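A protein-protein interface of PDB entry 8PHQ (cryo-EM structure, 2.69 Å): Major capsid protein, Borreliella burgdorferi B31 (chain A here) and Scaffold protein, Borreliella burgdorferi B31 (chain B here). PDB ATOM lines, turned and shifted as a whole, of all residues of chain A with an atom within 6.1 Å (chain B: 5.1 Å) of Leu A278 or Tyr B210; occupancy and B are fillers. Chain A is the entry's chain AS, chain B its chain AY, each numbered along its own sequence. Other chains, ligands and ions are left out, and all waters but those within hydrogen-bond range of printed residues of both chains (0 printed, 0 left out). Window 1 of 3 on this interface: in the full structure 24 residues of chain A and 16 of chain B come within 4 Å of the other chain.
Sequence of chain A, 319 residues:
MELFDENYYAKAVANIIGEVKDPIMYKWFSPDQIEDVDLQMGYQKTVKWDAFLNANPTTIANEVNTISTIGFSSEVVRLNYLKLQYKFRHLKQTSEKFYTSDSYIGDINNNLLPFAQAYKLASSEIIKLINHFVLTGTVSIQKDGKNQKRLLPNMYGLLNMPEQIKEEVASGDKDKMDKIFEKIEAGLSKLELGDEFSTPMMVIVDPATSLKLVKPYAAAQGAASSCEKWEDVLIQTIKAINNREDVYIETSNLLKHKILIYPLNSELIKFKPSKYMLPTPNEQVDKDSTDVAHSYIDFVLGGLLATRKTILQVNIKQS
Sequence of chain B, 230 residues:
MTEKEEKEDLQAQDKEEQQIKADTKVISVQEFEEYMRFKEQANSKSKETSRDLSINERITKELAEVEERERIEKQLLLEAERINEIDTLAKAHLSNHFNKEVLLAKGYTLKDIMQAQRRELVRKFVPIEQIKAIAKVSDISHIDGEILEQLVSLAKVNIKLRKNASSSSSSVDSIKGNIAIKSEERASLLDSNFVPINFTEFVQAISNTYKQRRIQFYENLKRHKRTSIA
O of Val A20 sits close to NH1 of Arg B213 (3.3 Å). NE of Arg B213 lies within salt-bridge range of OD1 of Asp A22, at 3.8 Å. The side-chain hydroxyl (OG) of Ser B207 is in hydrogen-bond range of the backbone carbonyl oxygen (O) of Lys A275 (3.4 Å). The backbone carbonyl oxygen of Pro A279 sits at hydrogen-bond distance from the side-chain hydroxyl of Tyr B210, at 3.3 Å.
OG of Ser A274 sits close to N of Tyr A276. The side-chain hydroxyl (OG1) of Thr A280 sits at hydrogen-bond distance from the backbone carbonyl oxygen (O) of Leu A278.
Among the printed residues, merely in contact across the chains: Ile A17 with Tyr B210 (3.3 Å), Leu A278 with Tyr B210 (3.4 Å), Tyr A26 with Arg B214 (3.5 Å) and Tyr A276 with Ser B207 (3.7 Å).
Printed residues of chain B within 4 Å of Ile A17: Tyr B210 (3.3 Å). Tyr A119 touches none of the printed residues of chain B. Ser A274 touches none of the printed residues of chain B. Of the printed residues of chain B, Lys A275 touches Ser B207. Printed residues of chain B within 4 Å of Pro A279: Tyr B210. Of the printed residues of chain A, Arg B213 touches Val A20 (2.2 Å) and Asp A22 (3.8 Å). The nearest printed residue of chain B that does not touch Leu A278 is Ile B206 (6.4 Å). The nearest residue of chain A that does not touch Tyr B210 is Tyr A119 (4.6 Å). The nearest printed residue of chain B that does not touch Tyr A276 is Tyr B210 (7.0 Å).
Of the 20 printed residues of chain A, 8 touch a printed residue of chain B. Printed residues of chain A that touch a printed residue of chain B: Ile A17, Val A20, Asp A22, Tyr A26, Lys A275, Tyr A276, Leu A278 and Pro A279. Hydrophobic or aromatic side chains of chain A that line the printed part of chain B: Ile A17, Tyr A26, Tyr A276 and Leu A278. Among the printed residues, Asp or Glu carboxylates within 4 Å of a Lys or Arg side-chain nitrogen of the other chain: Asp A22 with Arg B213 (3.8 Å).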
ATOM      1  N   ILE A  17      -6.011  25.338 -26.844  1.00  0.00           N
ATOM      2  CA  ILE A  17      -7.262  25.237 -26.097  1.00  0.00           C
ATOM      3  C   ILE A  17      -7.008  25.095 -24.602  1.00  0.00           C
ATOM      4  O   ILE A  17      -7.836  25.506 -23.781  1.00  0.00           O
ATOM      5  CB  ILE A  17      -8.107  24.066 -26.641  1.00  0.00           C
ATOM      6  CG1 ILE A  17      -9.498  24.059 -26.004  1.00  0.00           C
ATOM      7  CG2 ILE A  17      -7.403  22.741 -26.403  1.00  0.00           C
ATOM      8  CD1 ILE A  17     -10.262  25.348 -26.201  1.00  0.00           C
ATOM      9  N   VAL A  20      -6.886  28.279 -21.803  1.00  0.00           N
ATOM     10  CA  VAL A  20      -8.082  28.966 -21.331  1.00  0.00           C
ATOM     11  C   VAL A  20      -8.429  28.480 -19.930  1.00  0.00           C
ATOM     12  O   VAL A  20      -8.392  27.277 -19.641  1.00  0.00           O
ATOM     13  CB  VAL A  20      -9.248  28.737 -22.307  1.00  0.00           C
ATOM     14  CG1 VAL A  20     -10.439  29.593 -21.921  1.00  0.00           C
ATOM     15  CG2 VAL A  20      -8.811  29.030 -23.732  1.00  0.00           C
ATOM     16  N   ASP A  22     -10.700  27.752 -16.472  1.00  0.00           N
ATOM     17  CA  ASP A  22     -12.000  27.154 -16.227  1.00  0.00           C
ATOM     18  C   ASP A  22     -13.029  28.229 -15.879  1.00  0.00           C
ATOM     19  O   ASP A  22     -12.699  29.234 -15.242  1.00  0.00           O
ATOM     20  CB  ASP A  22     -11.919  26.137 -15.093  1.00  0.00           C
ATOM     21  CG  ASP A  22     -11.234  24.852 -15.509  1.00  0.00           C
ATOM     22  OD1 ASP A  22     -11.716  24.203 -16.460  1.00  0.00           O
ATOM     23  OD2 ASP A  22     -10.216  24.489 -14.884  1.00  0.00           O
ATOM     24  N   PRO A  23     -14.280  28.048 -16.298  1.00  0.00           N
ATOM     25  CA  PRO A  23     -15.330  28.996 -15.914  1.00  0.00           C
ATOM     26  C   PRO A  23     -15.512  29.026 -14.404  1.00  0.00           C
ATOM     27  O   PRO A  23     -15.399  28.003 -13.727  1.00  0.00           O
ATOM     28  CB  PRO A  23     -16.575  28.446 -16.617  1.00  0.00           C
ATOM     29  CG  PRO A  23     -16.035  27.670 -17.767  1.00  0.00           C
ATOM     30  CD  PRO A  23     -14.774  27.042 -17.253  1.00  0.00           C
ATOM     31  N   MET A  25     -18.313  29.632 -12.992  1.00  0.00           N
ATOM     32  CA  MET A  25     -19.655  29.177 -12.651  1.00  0.00           C
ATOM     33  C   MET A  25     -19.650  27.771 -12.074  1.00  0.00           C
ATOM     34  O   MET A  25     -20.626  27.376 -11.430  1.00  0.00           O
ATOM     35  CB  MET A  25     -20.565  29.213 -13.877  1.00  0.00           C
ATOM     36  CG  MET A  25     -19.904  28.736 -15.151  1.00  0.00           C
ATOM     37  SD  MET A  25     -21.014  28.803 -16.567  1.00  0.00           S
ATOM     38  CE  MET A  25     -20.145  27.756 -17.725  1.00  0.00           C
ATOM     39  N   TYR A  26     -18.579  27.010 -12.298  1.00  0.00           N
ATOM     40  CA  TYR A  26     -18.487  25.658 -11.768  1.00  0.00           C
ATOM     41  C   TYR A  26     -18.430  25.637 -10.247  1.00  0.00           C
ATOM     42  O   TYR A  26     -18.702  24.594  -9.644  1.00  0.00           O
ATOM     43  CB  TYR A  26     -17.255  24.960 -12.344  1.00  0.00           C
ATOM     44  CG  TYR A  26     -17.356  24.611 -13.810  1.00  0.00           C
ATOM     45  CD1 TYR A  26     -18.543  24.778 -14.506  1.00  0.00           C
ATOM     46  CD2 TYR A  26     -16.254  24.129 -14.500  1.00  0.00           C
ATOM     47  CE1 TYR A  26     -18.634  24.461 -15.845  1.00  0.00           C
ATOM     48  CE2 TYR A  26     -16.334  23.814 -15.839  1.00  0.00           C
ATOM     49  CZ  TYR A  26     -17.526  23.981 -16.506  1.00  0.00           C
ATOM     50  OH  TYR A  26     -17.610  23.666 -17.842  1.00  0.00           O
ATOM     51  N   TYR A 119      -7.700  34.036 -30.430  1.00  0.00           N
ATOM     52  CA  TYR A 119      -8.721  33.071 -30.048  1.00  0.00           C
ATOM     53  C   TYR A 119      -8.763  32.876 -28.542  1.00  0.00           C
ATOM     54  O   TYR A 119      -9.845  32.826 -27.950  1.00  0.00           O
ATOM     55  CB  TYR A 119      -8.461  31.738 -30.744  1.00  0.00           C
ATOM     56  CG  TYR A 119      -9.449  30.665 -30.368  1.00  0.00           C
ATOM     57  CD1 TYR A 119     -10.767  30.725 -30.797  1.00  0.00           C
ATOM     58  CD2 TYR A 119      -9.073  29.607 -29.554  1.00  0.00           C
ATOM     59  CE1 TYR A 119     -11.674  29.750 -30.446  1.00  0.00           C
ATOM     60  CE2 TYR A 119      -9.974  28.630 -29.196  1.00  0.00           C
ATOM     61  CZ  TYR A 119     -11.273  28.706 -29.644  1.00  0.00           C
ATOM     62  OH  TYR A 119     -12.174  27.733 -29.288  1.00  0.00           O
ATOM     63  N   SER A 123     -12.002  33.852 -26.330  1.00  0.00           N
ATOM     64  CA  SER A 123     -12.665  32.790 -25.586  1.00  0.00           C
ATOM     65  C   SER A 123     -12.787  33.148 -24.114  1.00  0.00           C
ATOM     66  O   SER A 123     -13.819  32.882 -23.491  1.00  0.00           O
ATOM     67  CB  SER A 123     -11.910  31.474 -25.756  1.00  0.00           C
ATOM     68  OG  SER A 123     -11.883  31.073 -27.113  1.00  0.00           O
ATOM     69  N   ILE A 127     -16.311  33.475 -22.145  1.00  0.00           N
ATOM     70  CA  ILE A 127     -16.573  32.680 -20.947  1.00  0.00           C
ATOM     71  C   ILE A 127     -17.041  33.568 -19.802  1.00  0.00           C
ATOM     72  O   ILE A 127     -17.946  33.199 -19.042  1.00  0.00           O
ATOM     73  CB  ILE A 127     -15.328  31.859 -20.564  1.00  0.00           C
ATOM     74  CG1 ILE A 127     -15.109  30.732 -21.573  1.00  0.00           C
ATOM     75  CG2 ILE A 127     -15.465  31.293 -19.164  1.00  0.00           C
ATOM     76  CD1 ILE A 127     -14.022  29.762 -21.182  1.00  0.00           C
ATOM     77  N   ILE A 130     -20.632  34.271 -20.409  1.00  0.00           N
ATOM     78  CA  ILE A 130     -21.460  33.113 -20.075  1.00  0.00           C
ATOM     79  C   ILE A 130     -21.652  33.004 -18.567  1.00  0.00           C
ATOM     80  O   ILE A 130     -22.745  32.676 -18.088  1.00  0.00           O
ATOM     81  CB  ILE A 130     -20.856  31.827 -20.666  1.00  0.00           C
ATOM     82  CG1 ILE A 130     -20.715  31.952 -22.183  1.00  0.00           C
ATOM     83  CG2 ILE A 130     -21.700  30.620 -20.304  1.00  0.00           C
ATOM     84  CD1 ILE A 130     -20.067  30.758 -22.841  1.00  0.00           C
ATOM     85  N   SER A 274     -26.000  22.781 -22.973  1.00  0.00           N
ATOM     86  CA  SER A 274     -25.583  22.150 -24.211  1.00  0.00           C
ATOM     87  C   SER A 274     -24.093  21.846 -24.143  1.00  0.00           C
ATOM     88  O   SER A 274     -23.315  22.584 -23.536  1.00  0.00           O
ATOM     89  CB  SER A 274     -25.885  23.058 -25.400  1.00  0.00           C
ATOM     90  OG  SER A 274     -25.179  22.643 -26.553  1.00  0.00           O
ATOM     91  N   LYS A 275     -23.693  20.739 -24.763  1.00  0.00           N
ATOM     92  CA  LYS A 275     -22.268  20.435 -24.772  1.00  0.00           C
ATOM     93  C   LYS A 275     -21.483  21.363 -25.684  1.00  0.00           C
ATOM     94  O   LYS A 275     -20.252  21.271 -25.724  1.00  0.00           O
ATOM     95  CB  LYS A 275     -22.032  18.978 -25.169  1.00  0.00           C
ATOM     96  CG  LYS A 275     -22.595  18.575 -26.512  1.00  0.00           C
ATOM     97  CD  LYS A 275     -22.292  17.111 -26.776  1.00  0.00           C
ATOM     98  CE  LYS A 275     -22.706  16.696 -28.171  1.00  0.00           C
ATOM     99  NZ  LYS A 275     -22.331  15.283 -28.452  1.00  0.00           N
ATOM    100  N   TYR A 276     -22.164  22.249 -26.410  1.00  0.00           N
ATOM    101  CA  TYR A 276     -21.533  23.289 -27.207  1.00  0.00           C
ATOM    102  C   TYR A 276     -21.619  24.657 -26.538  1.00  0.00           C
ATOM    103  O   TYR A 276     -21.416  25.677 -27.202  1.00  0.00           O
ATOM    104  CB  TYR A 276     -22.171  23.338 -28.595  1.00  0.00           C
ATOM    105  CG  TYR A 276     -22.277  21.984 -29.252  1.00  0.00           C
ATOM    106  CD1 TYR A 276     -21.141  21.283 -29.627  1.00  0.00           C
ATOM    107  CD2 TYR A 276     -23.514  21.399 -29.480  1.00  0.00           C
ATOM    108  CE1 TYR A 276     -21.235  20.043 -30.224  1.00  0.00           C
ATOM    109  CE2 TYR A 276     -23.617  20.159 -30.073  1.00  0.00           C
ATOM    110  CZ  TYR A 276     -22.475  19.485 -30.443  1.00  0.00           C
ATOM    111  OH  TYR A 276     -22.574  18.250 -31.036  1.00  0.00           O
ATOM    112  N   MET A 277     -21.925  24.695 -25.237  1.00  0.00           N
ATOM    113  CA  MET A 277     -22.116  25.971 -24.554  1.00  0.00           C
ATOM    114  C   MET A 277     -20.833  26.791 -24.533  1.00  0.00           C
ATOM    115  O   MET A 277     -20.859  28.005 -24.763  1.00  0.00           O
ATOM    116  CB  MET A 277     -22.613  25.736 -23.128  1.00  0.00           C
ATOM    117  CG  MET A 277     -22.250  26.852 -22.159  1.00  0.00           C
ATOM    118  SD  MET A 277     -22.878  26.602 -20.491  1.00  0.00           S
ATOM    119  CE  MET A 277     -21.760  25.331 -19.909  1.00  0.00           C
ATOM    120  N   LEU A 278     -19.706  26.152 -24.251  1.00  0.00           N
ATOM    121  CA  LEU A 278     -18.441  26.856 -24.176  1.00  0.00           C
ATOM    122  C   LEU A 278     -17.942  27.203 -25.577  1.00  0.00           C
ATOM    123  O   LEU A 278     -18.324  26.558 -26.556  1.00  0.00           O
ATOM    124  CB  LEU A 278     -17.426  26.006 -23.419  1.00  0.00           C
ATOM    125  CG  LEU A 278     -17.734  25.916 -21.921  1.00  0.00           C
ATOM    126  CD1 LEU A 278     -16.577  25.323 -21.146  1.00  0.00           C
ATOM    127  CD2 LEU A 278     -18.102  27.282 -21.361  1.00  0.00           C
ATOM    128  N   PRO A 279     -17.098  28.231 -25.699  1.00  0.00           N
ATOM    129  CA  PRO A 279     -16.725  28.731 -27.030  1.00  0.00           C
ATOM    130  C   PRO A 279     -16.131  27.648 -27.919  1.00  0.00           C
ATOM    131  O   PRO A 279     -15.324  26.826 -27.482  1.00  0.00           O
ATOM    132  CB  PRO A 279     -15.696  29.819 -26.714  1.00  0.00           C
ATOM    133  CG  PRO A 279     -16.099  30.319 -25.379  1.00  0.00           C
ATOM    134  CD  PRO A 279     -16.607  29.118 -24.629  1.00  0.00           C
ATOM    135  N   THR A 280     -16.543  27.660 -29.189  1.00  0.00           N
ATOM    136  CA  THR A 280     -16.103  26.677 -30.169  1.00  0.00           C
ATOM    137  C   THR A 280     -15.832  27.404 -31.482  1.00  0.00           C
ATOM    138  O   THR A 280     -16.646  28.241 -31.900  1.00  0.00           O
ATOM    139  CB  THR A 280     -17.160  25.583 -30.364  1.00  0.00           C
ATOM    140  OG1 THR A 280     -17.342  24.869 -29.135  1.00  0.00           O
ATOM    141  CG2 THR A 280     -16.746  24.608 -31.454  1.00  0.00           C
ATOM    142  N   ASP A 298     -18.562  30.369 -31.702  1.00  0.00           N
ATOM    143  CA  ASP A 298     -19.936  29.985 -31.417  1.00  0.00           C
ATOM    144  C   ASP A 298     -20.069  29.583 -29.955  1.00  0.00           C
ATOM    145  O   ASP A 298     -19.160  28.965 -29.389  1.00  0.00           O
ATOM    146  CB  ASP A 298     -20.367  28.804 -32.291  1.00  0.00           C
ATOM    147  CG  ASP A 298     -20.485  29.165 -33.754  1.00  0.00           C
ATOM    148  OD1 ASP A 298     -20.788  30.334 -34.058  1.00  0.00           O
ATOM    149  OD2 ASP A 298     -20.272  28.274 -34.602  1.00  0.00           O
ATOM    150  N   PHE A 299     -21.205  29.924 -29.350  1.00  0.00           N
ATOM    151  CA  PHE A 299     -21.534  29.425 -28.021  1.00  0.00           C
ATOM    152  C   PHE A 299     -23.047  29.321 -27.885  1.00  0.00           C
ATOM    153  O   PHE A 299     -23.801  29.849 -28.703  1.00  0.00           O
ATOM    154  CB  PHE A 299     -20.926  30.286 -26.902  1.00  0.00           C
ATOM    155  CG  PHE A 299     -21.279  31.746 -26.968  1.00  0.00           C
ATOM    156  CD1 PHE A 299     -20.767  32.559 -27.964  1.00  0.00           C
ATOM    157  CD2 PHE A 299     -22.106  32.309 -26.013  1.00  0.00           C
ATOM    158  CE1 PHE A 299     -21.083  33.899 -28.011  1.00  0.00           C
ATOM    159  CE2 PHE A 299     -22.425  33.647 -26.058  1.00  0.00           C
ATOM    160  CZ  PHE A 299     -21.914  34.443 -27.057  1.00  0.00           C
ATOM    161  N   VAL A 300     -23.485  28.580 -26.869  1.00  0.00           N
ATOM    162  CA  VAL A 300     -24.898  28.274 -26.667  1.00  0.00           C
ATOM    163  C   VAL A 300     -25.277  28.611 -25.232  1.00  0.00           C
ATOM    164  O   VAL A 300     -24.559  28.251 -24.294  1.00  0.00           O
ATOM    165  CB  VAL A 300     -25.213  26.797 -26.976  1.00  0.00           C
ATOM    166  CG1 VAL A 300     -26.684  26.512 -26.754  1.00  0.00           C
ATOM    167  CG2 VAL A 300     -24.819  26.456 -28.402  1.00  0.00           C
ATOM    168  N   ALA B 205     -14.238  16.538 -30.238  1.00  0.00           N
ATOM    169  CA  ALA B 205     -13.063  16.477 -29.376  1.00  0.00           C
ATOM    170  C   ALA B 205     -12.997  17.680 -28.445  1.00  0.00           C
ATOM    171  O   ALA B 205     -12.647  17.540 -27.268  1.00  0.00           O
ATOM    172  CB  ALA B 205     -11.796  16.382 -30.224  1.00  0.00           C
ATOM    173  N   ILE B 206     -13.323  18.871 -28.953  1.00  0.00           N
ATOM    174  CA  ILE B 206     -13.323  20.059 -28.099  1.00  0.00           C
ATOM    175  C   ILE B 206     -14.359  19.923 -26.987  1.00  0.00           C
ATOM    176  O   ILE B 206     -14.099  20.265 -25.823  1.00  0.00           O
ATOM    177  CB  ILE B 206     -13.558  21.329 -28.936  1.00  0.00           C
ATOM    178  CG1 ILE B 206     -12.455  21.501 -29.979  1.00  0.00           C
ATOM    179  CG2 ILE B 206     -13.625  22.553 -28.044  1.00  0.00           C
ATOM    180  CD1 ILE B 206     -12.589  22.766 -30.787  1.00  0.00           C
ATOM    181  N   SER B 207     -15.552  19.430 -27.327  1.00  0.00           N
ATOM    182  CA  SER B 207     -16.589  19.255 -26.311  1.00  0.00           C
ATOM    183  C   SER B 207     -16.153  18.260 -25.241  1.00  0.00           C
ATOM    184  O   SER B 207     -16.340  18.499 -24.038  1.00  0.00           O
ATOM    185  CB  SER B 207     -17.892  18.800 -26.967  1.00  0.00           C
ATOM    186  OG  SER B 207     -18.284  19.694 -27.991  1.00  0.00           O
ATOM    187  N   ASN B 208     -15.553  17.143 -25.658  1.00  0.00           N
ATOM    188  CA  ASN B 208     -15.079  16.162 -24.690  1.00  0.00           C
ATOM    189  C   ASN B 208     -13.956  16.729 -23.830  1.00  0.00           C
ATOM    190  O   ASN B 208     -13.869  16.426 -22.635  1.00  0.00           O
ATOM    191  CB  ASN B 208     -14.628  14.891 -25.408  1.00  0.00           C
ATOM    192  CG  ASN B 208     -15.764  14.203 -26.139  1.00  0.00           C
ATOM    193  OD1 ASN B 208     -16.908  14.656 -26.100  1.00  0.00           O
ATOM    194  ND2 ASN B 208     -15.454  13.103 -26.811  1.00  0.00           N
ATOM    195  N   THR B 209     -13.087  17.554 -24.419  1.00  0.00           N
ATOM    196  CA  THR B 209     -12.029  18.190 -23.642  1.00  0.00           C
ATOM    197  C   THR B 209     -12.608  19.091 -22.560  1.00  0.00           C
ATOM    198  O   THR B 209     -12.153  19.064 -21.409  1.00  0.00           O
ATOM    199  CB  THR B 209     -11.108  18.989 -24.563  1.00  0.00           C
ATOM    200  OG1 THR B 209     -10.569  18.121 -25.566  1.00  0.00           O
ATOM    201  CG2 THR B 209      -9.968  19.609 -23.773  1.00  0.00           C
ATOM    202  N   TYR B 210     -13.619  19.891 -22.907  1.00  0.00           N
ATOM    203  CA  TYR B 210     -14.249  20.738 -21.896  1.00  0.00           C
ATOM    204  C   TYR B 210     -14.887  19.900 -20.793  1.00  0.00           C
ATOM    205  O   TYR B 210     -14.779  20.234 -19.605  1.00  0.00           O
ATOM    206  CB  TYR B 210     -15.288  21.658 -22.535  1.00  0.00           C
ATOM    207  CG  TYR B 210     -14.713  22.879 -23.214  1.00  0.00           C
ATOM    208  CD1 TYR B 210     -13.873  23.745 -22.528  1.00  0.00           C
ATOM    209  CD2 TYR B 210     -15.043  23.191 -24.524  1.00  0.00           C
ATOM    210  CE1 TYR B 210     -13.358  24.870 -23.134  1.00  0.00           C
ATOM    211  CE2 TYR B 210     -14.533  24.315 -25.140  1.00  0.00           C
ATOM    212  CZ  TYR B 210     -13.691  25.150 -24.442  1.00  0.00           C
ATOM    213  OH  TYR B 210     -13.181  26.272 -25.052  1.00  0.00           O
ATOM    214  N   LYS B 211     -15.551  18.803 -21.165  1.00  0.00           N
ATOM    215  CA  LYS B 211     -16.171  17.947 -20.155  1.00  0.00           C
ATOM    216  C   LYS B 211     -15.127  17.358 -19.210  1.00  0.00           C
ATOM    217  O   LYS B 211     -15.315  17.349 -17.984  1.00  0.00           O
ATOM    218  CB  LYS B 211     -16.974  16.839 -20.837  1.00  0.00           C
ATOM    219  CG  LYS B 211     -17.574  15.818 -19.887  1.00  0.00           C
ATOM    220  CD  LYS B 211     -18.279  14.713 -20.655  1.00  0.00           C
ATOM    221  CE  LYS B 211     -18.874  13.679 -19.716  1.00  0.00           C
ATOM    222  NZ  LYS B 211     -19.591  12.606 -20.457  1.00  0.00           N
ATOM    223  N   GLN B 212     -14.011  16.875 -19.760  1.00  0.00           N
ATOM    224  CA  GLN B 212     -12.967  16.298 -18.919  1.00  0.00           C
ATOM    225  C   GLN B 212     -12.335  17.348 -18.017  1.00  0.00           C
ATOM    226  O   GLN B 212     -11.990  17.055 -16.866  1.00  0.00           O
ATOM    227  CB  GLN B 212     -11.907  15.616 -19.781  1.00  0.00           C
ATOM    228  CG  GLN B 212     -12.444  14.478 -20.629  1.00  0.00           C
ATOM    229  CD  GLN B 212     -11.399  13.905 -21.560  1.00  0.00           C
ATOM    230  OE1 GLN B 212     -10.246  14.336 -21.556  1.00  0.00           O
ATOM    231  NE2 GLN B 212     -11.797  12.932 -22.370  1.00  0.00           N
ATOM    232  N   ARG B 213     -12.166  18.575 -18.515  1.00  0.00           N
ATOM    233  CA  ARG B 213     -11.638  19.632 -17.658  1.00  0.00           C
ATOM    234  C   ARG B 213     -12.595  19.951 -16.518  1.00  0.00           C
ATOM    235  O   ARG B 213     -12.161  20.220 -15.393  1.00  0.00           O
ATOM    236  CB  ARG B 213     -11.334  20.888 -18.470  1.00  0.00           C
ATOM    237  CG  ARG B 213     -10.271  20.700 -19.533  1.00  0.00           C
ATOM    238  CD  ARG B 213      -9.169  21.725 -19.364  1.00  0.00           C
ATOM    239  NE  ARG B 213      -9.687  23.081 -19.490  1.00  0.00           N
ATOM    240  CZ  ARG B 213      -8.954  24.179 -19.371  1.00  0.00           C
ATOM    241  NH1 ARG B 213      -7.655  24.119 -19.119  1.00  0.00           N
ATOM    242  NH2 ARG B 213      -9.537  25.366 -19.502  1.00  0.00           N
ATOM    243  N   ARG B 214     -13.903  19.933 -16.786  1.00  0.00           N
ATOM    244  CA  ARG B 214     -14.870  20.134 -15.708  1.00  0.00           C
ATOM    245  C   ARG B 214     -14.758  19.038 -14.651  1.00  0.00           C
ATOM    246  O   ARG B 214     -14.771  19.319 -13.441  1.00  0.00           O
ATOM    247  CB  ARG B 214     -16.285  20.177 -16.278  1.00  0.00           C
ATOM    248  CG  ARG B 214     -17.361  20.507 -15.262  1.00  0.00           C
ATOM    249  CD  ARG B 214     -18.634  19.775 -15.609  1.00  0.00           C
ATOM    250  NE  ARG B 214     -18.945  19.905 -17.026  1.00  0.00           N
ATOM    251  CZ  ARG B 214     -19.924  19.259 -17.643  1.00  0.00           C
ATOM    252  NH1 ARG B 214     -20.700  18.403 -16.999  1.00  0.00           N
ATOM    253  NH2 ARG B 214     -20.120  19.467 -18.941  1.00  0.00           N
